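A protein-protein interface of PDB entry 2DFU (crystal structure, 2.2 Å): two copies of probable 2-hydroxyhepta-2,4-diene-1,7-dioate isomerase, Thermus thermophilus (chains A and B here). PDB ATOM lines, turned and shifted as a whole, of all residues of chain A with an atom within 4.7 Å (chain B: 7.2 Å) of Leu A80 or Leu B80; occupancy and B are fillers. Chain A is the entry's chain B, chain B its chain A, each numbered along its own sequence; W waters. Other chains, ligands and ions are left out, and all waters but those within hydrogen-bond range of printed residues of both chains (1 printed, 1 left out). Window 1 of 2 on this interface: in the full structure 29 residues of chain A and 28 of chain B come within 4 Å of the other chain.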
ATOM      1  N   ILE A  50      14.387   4.142  19.579  1.00  0.00           N
ATOM      2  CA  ILE A  50      13.789   2.854  19.283  1.00  0.00           C
ATOM      3  C   ILE A  50      14.843   1.774  19.531  1.00  0.00           C
ATOM      4  O   ILE A  50      15.879   1.737  18.863  1.00  0.00           O
ATOM      5  CB  ILE A  50      13.310   2.816  17.825  1.00  0.00           C
ATOM      6  CG1 ILE A  50      12.339   3.980  17.586  1.00  0.00           C
ATOM      7  CG2 ILE A  50      12.616   1.491  17.531  1.00  0.00           C
ATOM      8  CD1 ILE A  50      12.060   4.264  16.138  1.00  0.00           C
ATOM      9  N   VAL A  51      14.580   0.915  20.511  1.00  0.00           N
ATOM     10  CA  VAL A  51      15.499  -0.164  20.879  1.00  0.00           C
ATOM     11  C   VAL A  51      14.960  -1.498  20.367  1.00  0.00           C
ATOM     12  O   VAL A  51      13.819  -1.865  20.643  1.00  0.00           O
ATOM     13  CB  VAL A  51      15.668  -0.241  22.414  1.00  0.00           C
ATOM     14  CG1 VAL A  51      16.775  -1.223  22.773  1.00  0.00           C
ATOM     15  CG2 VAL A  51      15.978   1.140  22.967  1.00  0.00           C
ATOM     16  N   LEU A  78      21.007  -6.210  21.261  1.00  0.00           N
ATOM     17  CA  LEU A  78      20.280  -4.980  20.972  1.00  0.00           C
ATOM     18  C   LEU A  78      20.872  -4.111  19.877  1.00  0.00           C
ATOM     19  O   LEU A  78      22.080  -4.099  19.670  1.00  0.00           O
ATOM     20  CB  LEU A  78      20.190  -4.132  22.240  1.00  0.00           C
ATOM     21  CG  LEU A  78      19.652  -4.762  23.522  1.00  0.00           C
ATOM     22  CD1 LEU A  78      19.828  -3.781  24.673  1.00  0.00           C
ATOM     23  CD2 LEU A  78      18.189  -5.125  23.340  1.00  0.00           C
ATOM     24  N   PHE A  79      20.006  -3.381  19.182  1.00  0.00           N
ATOM     25  CA  PHE A  79      20.439  -2.448  18.147  1.00  0.00           C
ATOM     26  C   PHE A  79      19.448  -1.292  18.126  1.00  0.00           C
ATOM     27  O   PHE A  79      18.309  -1.441  18.564  1.00  0.00           O
ATOM     28  CB  PHE A  79      20.560  -3.115  16.760  1.00  0.00           C
ATOM     29  CG  PHE A  79      19.263  -3.631  16.185  1.00  0.00           C
ATOM     30  CD1 PHE A  79      18.813  -4.917  16.480  1.00  0.00           C
ATOM     31  CD2 PHE A  79      18.527  -2.855  15.288  1.00  0.00           C
ATOM     32  CE1 PHE A  79      17.653  -5.430  15.883  1.00  0.00           C
ATOM     33  CE2 PHE A  79      17.367  -3.356  14.687  1.00  0.00           C
ATOM     34  CZ  PHE A  79      16.931  -4.651  14.985  1.00  0.00           C
ATOM     35  N   LEU A  80      19.884  -0.137  17.635  1.00  0.00           N
ATOM     36  CA  LEU A  80      19.032   1.046  17.611  1.00  0.00           C
ATOM     37  C   LEU A  80      18.553   1.478  16.238  1.00  0.00           C
ATOM     38  O   LEU A  80      19.219   1.248  15.227  1.00  0.00           O
ATOM     39  CB  LEU A  80      19.765   2.233  18.241  1.00  0.00           C
ATOM     40  CG  LEU A  80      20.130   2.200  19.726  1.00  0.00           C
ATOM     41  CD1 LEU A  80      21.073   3.365  20.059  1.00  0.00           C
ATOM     42  CD2 LEU A  80      18.860   2.278  20.556  1.00  0.00           C
ATOM     43  N   LYS A  81      17.383   2.109  16.225  1.00  0.00           N
ATOM     44  CA  LYS A  81      16.800   2.666  15.014  1.00  0.00           C
ATOM     45  C   LYS A  81      16.478   4.110  15.382  1.00  0.00           C
ATOM     46  O   LYS A  81      16.002   4.377  16.479  1.00  0.00           O
ATOM     47  CB  LYS A  81      15.498   1.959  14.619  1.00  0.00           C
ATOM     48  CG  LYS A  81      15.636   0.617  13.897  1.00  0.00           C
ATOM     49  CD  LYS A  81      14.237   0.076  13.546  1.00  0.00           C
ATOM     50  CE  LYS A  81      14.253  -1.311  12.897  1.00  0.00           C
ATOM     51  NZ  LYS A  81      14.566  -1.275  11.431  1.00  0.00           N
ATOM     52  N   GLY A  82      16.756   5.042  14.480  1.00  0.00           N
ATOM     53  CA  GLY A  82      16.435   6.429  14.753  1.00  0.00           C
ATOM     54  C   GLY A  82      14.973   6.639  14.403  1.00  0.00           C
ATOM     55  O   GLY A  82      14.402   5.830  13.670  1.00  0.00           O
ATOM     56  N   VAL A 159      23.681   0.884  11.258  1.00  0.00           N
ATOM     57  CA  VAL A 159      22.975   2.144  11.052  1.00  0.00           C
ATOM     58  C   VAL A 159      22.233   2.183   9.719  1.00  0.00           C
ATOM     59  O   VAL A 159      21.019   2.379   9.672  1.00  0.00           O
ATOM     60  CB  VAL A 159      23.950   3.340  11.115  1.00  0.00           C
ATOM     61  CG1 VAL A 159      23.199   4.639  10.872  1.00  0.00           C
ATOM     62  CG2 VAL A 159      24.632   3.373  12.470  1.00  0.00           C
ATOM     63  N   SER A 163      18.520   1.450  10.206  1.00  0.00           N
ATOM     64  CA  SER A 163      17.945   2.763  10.479  1.00  0.00           C
ATOM     65  C   SER A 163      17.815   3.738   9.312  1.00  0.00           C
ATOM     66  O   SER A 163      17.745   4.952   9.520  1.00  0.00           O
ATOM     67  CB  SER A 163      18.730   3.426  11.614  1.00  0.00           C
ATOM     68  OG  SER A 163      17.987   4.484  12.195  1.00  0.00           O
ATOM     69  N   MET A 217      20.244   1.766  30.311  1.00  0.00           N
ATOM     70  CA  MET A 217      19.590   2.762  29.467  1.00  0.00           C
ATOM     71  C   MET A 217      18.167   3.076  29.917  1.00  0.00           C
ATOM     72  O   MET A 217      17.304   2.199  29.946  1.00  0.00           O
ATOM     73  CB  MET A 217      19.586   2.264  28.017  1.00  0.00           C
ATOM     74  CG  MET A 217      18.584   2.948  27.100  1.00  0.00           C
ATOM     75  SD  MET A 217      18.628   2.263  25.417  1.00  0.00           S
ATOM     76  CE  MET A 217      19.980   3.222  24.705  1.00  0.00           C
ATOM     77  N   LYS B  49      17.894  12.226  17.336  1.00  0.00           N
ATOM     78  CA  LYS B  49      18.878  11.146  17.299  1.00  0.00           C
ATOM     79  C   LYS B  49      20.297  11.705  17.231  1.00  0.00           C
ATOM     80  O   LYS B  49      20.498  12.862  16.869  1.00  0.00           O
ATOM     81  CB  LYS B  49      18.618  10.231  16.098  1.00  0.00           C
ATOM     82  CG  LYS B  49      18.689  10.929  14.751  1.00  0.00           C
ATOM     83  CD  LYS B  49      18.348   9.958  13.625  1.00  0.00           C
ATOM     84  CE  LYS B  49      18.410  10.639  12.263  1.00  0.00           C
ATOM     85  NZ  LYS B  49      17.378  11.694  12.162  1.00  0.00           N
ATOM     86  N   ILE B  50      21.275  10.879  17.582  1.00  0.00           N
ATOM     87  CA  ILE B  50      22.675  11.294  17.574  1.00  0.00           C
ATOM     88  C   ILE B  50      23.482  10.317  16.732  1.00  0.00           C
ATOM     89  O   ILE B  50      23.611   9.142  17.082  1.00  0.00           O
ATOM     90  CB  ILE B  50      23.218  11.334  19.014  1.00  0.00           C
ATOM     91  CG1 ILE B  50      22.421  12.368  19.818  1.00  0.00           C
ATOM     92  CG2 ILE B  50      24.707  11.675  19.023  1.00  0.00           C
ATOM     93  CD1 ILE B  50      22.354  12.080  21.296  1.00  0.00           C
ATOM     94  N   VAL B  51      24.009  10.802  15.608  1.00  0.00           N
ATOM     95  CA  VAL B  51      24.789   9.970  14.695  1.00  0.00           C
ATOM     96  C   VAL B  51      26.279  10.203  14.923  1.00  0.00           C
ATOM     97  O   VAL B  51      26.742  11.344  14.939  1.00  0.00           O
ATOM     98  CB  VAL B  51      24.426  10.290  13.226  1.00  0.00           C
ATOM     99  CG1 VAL B  51      25.086   9.298  12.299  1.00  0.00           C
ATOM    100  CG2 VAL B  51      22.913  10.254  13.047  1.00  0.00           C
ATOM    101  N   CYS B  52      27.038   9.124  15.095  1.00  0.00           N
ATOM    102  CA  CYS B  52      28.462   9.273  15.364  1.00  0.00           C
ATOM    103  C   CYS B  52      29.372   8.578  14.366  1.00  0.00           C
ATOM    104  O   CYS B  52      29.050   7.515  13.847  1.00  0.00           O
ATOM    105  CB  CYS B  52      28.768   8.755  16.764  1.00  0.00           C
ATOM    106  SG  CYS B  52      27.481   9.157  17.962  1.00  0.00           S
ATOM    107  N   LEU B  78      29.598   4.472  10.946  1.00  0.00           N
ATOM    108  CA  LEU B  78      28.649   5.172  11.808  1.00  0.00           C
ATOM    109  C   LEU B  78      28.017   4.331  12.908  1.00  0.00           C
ATOM    110  O   LEU B  78      27.932   3.107  12.804  1.00  0.00           O
ATOM    111  CB  LEU B  78      27.515   5.750  10.962  1.00  0.00           C
ATOM    112  CG  LEU B  78      27.843   6.640   9.761  1.00  0.00           C
ATOM    113  CD1 LEU B  78      26.578   6.840   8.938  1.00  0.00           C
ATOM    114  CD2 LEU B  78      28.400   7.978  10.218  1.00  0.00           C
ATOM    115  N   PHE B  79      27.581   5.002  13.969  1.00  0.00           N
ATOM    116  CA  PHE B  79      26.879   4.345  15.062  1.00  0.00           C
ATOM    117  C   PHE B  79      25.975   5.372  15.729  1.00  0.00           C
ATOM    118  O   PHE B  79      26.203   6.582  15.618  1.00  0.00           O
ATOM    119  CB  PHE B  79      27.838   3.695  16.076  1.00  0.00           C
ATOM    120  CG  PHE B  79      28.751   4.654  16.782  1.00  0.00           C
ATOM    121  CD1 PHE B  79      29.986   4.989  16.238  1.00  0.00           C
ATOM    122  CD2 PHE B  79      28.400   5.179  18.021  1.00  0.00           C
ATOM    123  CE1 PHE B  79      30.864   5.833  16.924  1.00  0.00           C
ATOM    124  CE2 PHE B  79      29.269   6.024  18.715  1.00  0.00           C
ATOM    125  CZ  PHE B  79      30.502   6.350  18.168  1.00  0.00           C
ATOM    126  N   LEU B  80      24.937   4.891  16.404  1.00  0.00           N
ATOM    127  CA  LEU B  80      23.973   5.773  17.058  1.00  0.00           C
ATOM    128  C   LEU B  80      24.070   5.811  18.574  1.00  0.00           C
ATOM    129  O   LEU B  80      24.580   4.892  19.211  1.00  0.00           O
ATOM    130  CB  LEU B  80      22.547   5.351  16.690  1.00  0.00           C
ATOM    131  CG  LEU B  80      22.187   5.272  15.207  1.00  0.00           C
ATOM    132  CD1 LEU B  80      20.874   4.509  15.051  1.00  0.00           C
ATOM    133  CD2 LEU B  80      22.073   6.678  14.611  1.00  0.00           C
ATOM    134  N   LYS B  81      23.565   6.900  19.135  1.00  0.00           N
ATOM    135  CA  LYS B  81      23.494   7.092  20.573  1.00  0.00           C
ATOM    136  C   LYS B  81      22.083   7.623  20.791  1.00  0.00           C
ATOM    137  O   LYS B  81      21.576   8.400  19.980  1.00  0.00           O
ATOM    138  CB  LYS B  81      24.529   8.116  21.057  1.00  0.00           C
ATOM    139  CG  LYS B  81      25.949   7.571  21.157  1.00  0.00           C
ATOM    140  CD  LYS B  81      26.973   8.694  21.312  1.00  0.00           C
ATOM    141  CE  LYS B  81      27.512   8.834  22.726  1.00  0.00           C
ATOM    142  NZ  LYS B  81      28.572   7.844  23.066  1.00  0.00           N
ATOM    143  N   GLY B  82      21.427   7.178  21.851  1.00  0.00           N
ATOM    144  CA  GLY B  82      20.092   7.672  22.116  1.00  0.00           C
ATOM    145  C   GLY B  82      20.203   8.956  22.912  1.00  0.00           C
ATOM    146  O   GLY B  82      21.254   9.221  23.487  1.00  0.00           O
ATOM    147  N   ASN B  84      19.217   9.612  25.685  1.00  0.00           N
ATOM    148  CA  ASN B  84      19.467   9.299  27.092  1.00  0.00           C
ATOM    149  C   ASN B  84      20.955   9.438  27.445  1.00  0.00           C
ATOM    150  O   ASN B  84      21.307   9.593  28.614  1.00  0.00           O
ATOM    151  CB  ASN B  84      19.020   7.873  27.404  1.00  0.00           C
ATOM    152  CG  ASN B  84      19.802   6.832  26.613  1.00  0.00           C
ATOM    153  OD1 ASN B  84      19.663   6.731  25.393  1.00  0.00           O
ATOM    154  ND2 ASN B  84      20.638   6.066  27.305  1.00  0.00           N
ATOM    155  N   GLN B 157      25.722  -5.215  19.183  1.00  0.00           N
ATOM    156  CA  GLN B 157      25.974  -3.873  18.669  1.00  0.00           C
ATOM    157  C   GLN B 157      26.449  -2.999  19.831  1.00  0.00           C
ATOM    158  O   GLN B 157      26.330  -3.385  20.998  1.00  0.00           O
ATOM    159  CB  GLN B 157      24.699  -3.281  18.051  1.00  0.00           C
ATOM    160  CG  GLN B 157      24.261  -3.945  16.742  1.00  0.00           C
ATOM    161  CD  GLN B 157      25.121  -3.537  15.555  1.00  0.00           C
ATOM    162  OE1 GLN B 157      25.053  -2.397  15.089  1.00  0.00           O
ATOM    163  NE2 GLN B 157      25.941  -4.465  15.067  1.00  0.00           N
ATOM    164  N   TRP B 158      26.971  -1.819  19.509  1.00  0.00           N
ATOM    165  CA  TRP B 158      27.499  -0.909  20.523  1.00  0.00           C
ATOM    166  C   TRP B 158      26.449  -0.139  21.319  1.00  0.00           C
ATOM    167  O   TRP B 158      26.662   1.027  21.662  1.00  0.00           O
ATOM    168  CB  TRP B 158      28.463   0.092  19.873  1.00  0.00           C
ATOM    169  CG  TRP B 158      29.599  -0.541  19.112  1.00  0.00           C
ATOM    170  CD1 TRP B 158      29.942  -1.869  19.088  1.00  0.00           C
ATOM    171  CD2 TRP B 158      30.538   0.129  18.264  1.00  0.00           C
ATOM    172  NE1 TRP B 158      31.035  -2.061  18.276  1.00  0.00           N
ATOM    173  CE2 TRP B 158      31.421  -0.854  17.758  1.00  0.00           C
ATOM    174  CE3 TRP B 158      30.720   1.464  17.880  1.00  0.00           C
ATOM    175  CZ2 TRP B 158      32.472  -0.540  16.886  1.00  0.00           C
ATOM    176  CZ3 TRP B 158      31.767   1.774  17.011  1.00  0.00           C
ATOM    177  CH2 TRP B 158      32.627   0.776  16.525  1.00  0.00           C
ATOM    178  N   VAL B 159      25.333  -0.781  21.644  1.00  0.00           N
ATOM    179  CA  VAL B 159      24.302  -0.085  22.393  1.00  0.00           C
ATOM    180  C   VAL B 159      24.731   0.293  23.812  1.00  0.00           C
ATOM    181  O   VAL B 159      24.731   1.478  24.157  1.00  0.00           O
ATOM    182  CB  VAL B 159      22.993  -0.886  22.437  1.00  0.00           C
ATOM    183  CG1 VAL B 159      21.936  -0.103  23.198  1.00  0.00           C
ATOM    184  CG2 VAL B 159      22.513  -1.149  21.019  1.00  0.00           C
ATOM    185  N   LYS B 162      28.165   2.474  23.819  1.00  0.00           N
ATOM    186  CA  LYS B 162      28.132   3.886  23.453  1.00  0.00           C
ATOM    187  C   LYS B 162      26.881   4.660  23.870  1.00  0.00           C
ATOM    188  O   LYS B 162      26.915   5.889  23.970  1.00  0.00           O
ATOM    189  CB  LYS B 162      28.267   4.012  21.930  1.00  0.00           C
ATOM    190  CG  LYS B 162      29.587   3.530  21.334  1.00  0.00           C
ATOM    191  CD  LYS B 162      30.680   4.581  21.515  1.00  0.00           C
ATOM    192  CE  LYS B 162      31.909   4.258  20.669  1.00  0.00           C
ATOM    193  NZ  LYS B 162      33.010   5.244  20.887  1.00  0.00           N
ATOM    194  N   SER B 163      25.782   3.955  24.109  1.00  0.00           N
ATOM    195  CA  SER B 163      24.538   4.633  24.426  1.00  0.00           C
ATOM    196  C   SER B 163      23.963   4.473  25.833  1.00  0.00           C
ATOM    197  O   SER B 163      22.757   4.645  26.036  1.00  0.00           O
ATOM    198  CB  SER B 163      23.487   4.236  23.390  1.00  0.00           C
ATOM    199  OG  SER B 163      22.397   5.140  23.405  1.00  0.00           O
ATOM    200  N   MET B 217      19.686   8.523   5.539  1.00  0.00           N
ATOM    201  CA  MET B 217      19.066   8.909   6.802  1.00  0.00           C
ATOM    202  C   MET B 217      18.827  10.410   6.864  1.00  0.00           C
ATOM    203  O   MET B 217      19.770  11.198   6.797  1.00  0.00           O
ATOM    204  CB  MET B 217      19.972   8.465   7.963  1.00  0.00           C
ATOM    205  CG  MET B 217      19.651   9.075   9.322  1.00  0.00           C
ATOM    206  SD  MET B 217      20.781   8.476  10.616  1.00  0.00           S
ATOM    207  CE  MET B 217      19.982   6.924  11.068  1.00  0.00           C
HETATM  208  O   HOH W   1      23.823  -5.380  21.495  1.00  0.00           O
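The backbone carbonyl oxygen (O) of Phe B79 is in hydrogen-bond range of the backbone NH (N) of Cys B52.
N of Gly B82 is in hydrogen-bond range of OG of Ser B163 (2.7 Å).
ND2 of Asn B84 is in hydrogen-bond range of O of Ser B163 (2.8 Å).
The side-chain hydroxyl (OG) of Ser A163 is in hydrogen-bond range of the backbone NH (N) of Gly A82 (2.7 Å).
Among the printed residues, pairs that only touch across the chains: Leu A78 with Gln B157 (3.2 Å), Leu A78 with Val B159 (3.3 Å), Val A159 with Leu B78 (3.3 Å), Ser A163 with Met B217 (3.3 Å), Met A217 with Ser B163 (3.3 Å), Val A159 with Phe B79 (3.6 Å), Met A217 with Asn B84 (3.6 Å), Leu A80 with Leu B80 (3.7 Å), Phe A79 with Val B159 (3.8 Å), Phe A79 with Gln B157 (3.8 Å) and Val A159 with Met B217 (3.95 Å).
Printed residues of chain B within 4 Å of Phe A79: Gln B157 (3.8 Å) and Val B159 (3.8 Å).
Printed residues of chain B within 4 Å of Leu A80: Leu B80.
Printed residues of chain B within 4 Å of Val A159: Leu B78 (3.3 Å), Phe B79 (3.6 Å) and Met B217 (3.95 Å).
Of the printed residues of chain B, Met A217 touches Asn B84 and Ser B163.
Of the printed residues of chain A, Phe B79 touches Val A159.
Leu B80 touches just one residue of chain A: Leu A80 (3.7 Å).
Lys B81 touches none of the printed residues of chain A.
Printed residues of chain A within 4 Å of Val B159: Leu A78 (3.3 Å) and Phe A79 (3.8 Å).
Printed residues of chain B that touch a printed residue of chain A: Leu B78, Phe B79, Leu B80, Asn B84, Gln B157, Val B159, Ser B163 and Met B217.
Hydrophobic or aromatic side chains of chain B that line the printed part of chain A: Leu B80, Val B159 and Met B217.
Along chain B the printed residues that touch a printed residue of chain A span positions 78 to 217.
Of the 10 printed residues of chain A, 6 touch a printed residue of chain B.
Printed residues of chain A that touch a printed residue of chain B: Leu A78, Phe A79, Leu A80, Val A159, Ser A163 and Met A217.
Among the printed residues, no Asp or Glu carboxylate lies within 4 Å of a Lys or Arg side-chain nitrogen of the other chain.
Leu A78 touches Val B159, and with the chains exchanged Val A159 touches Leu B78.
Phe A79 touches Val B159, and with the chains exchanged Val A159 touches Phe B79.
Val A159 touches Met B217, but with the chains exchanged Met A217 does not touch Val B159 (4.1 Å).
Ser A163 touches Met B217, and with the chains exchanged Met A217 touches Ser B163.
Of the 11 pairs that touch across the chains among the printed residues, 7 have their exchanged pair printed and touching as well.
Water W1 bridges O of Leu A78 (2.8 Å) and N of Gln B157 (3.0 Å).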
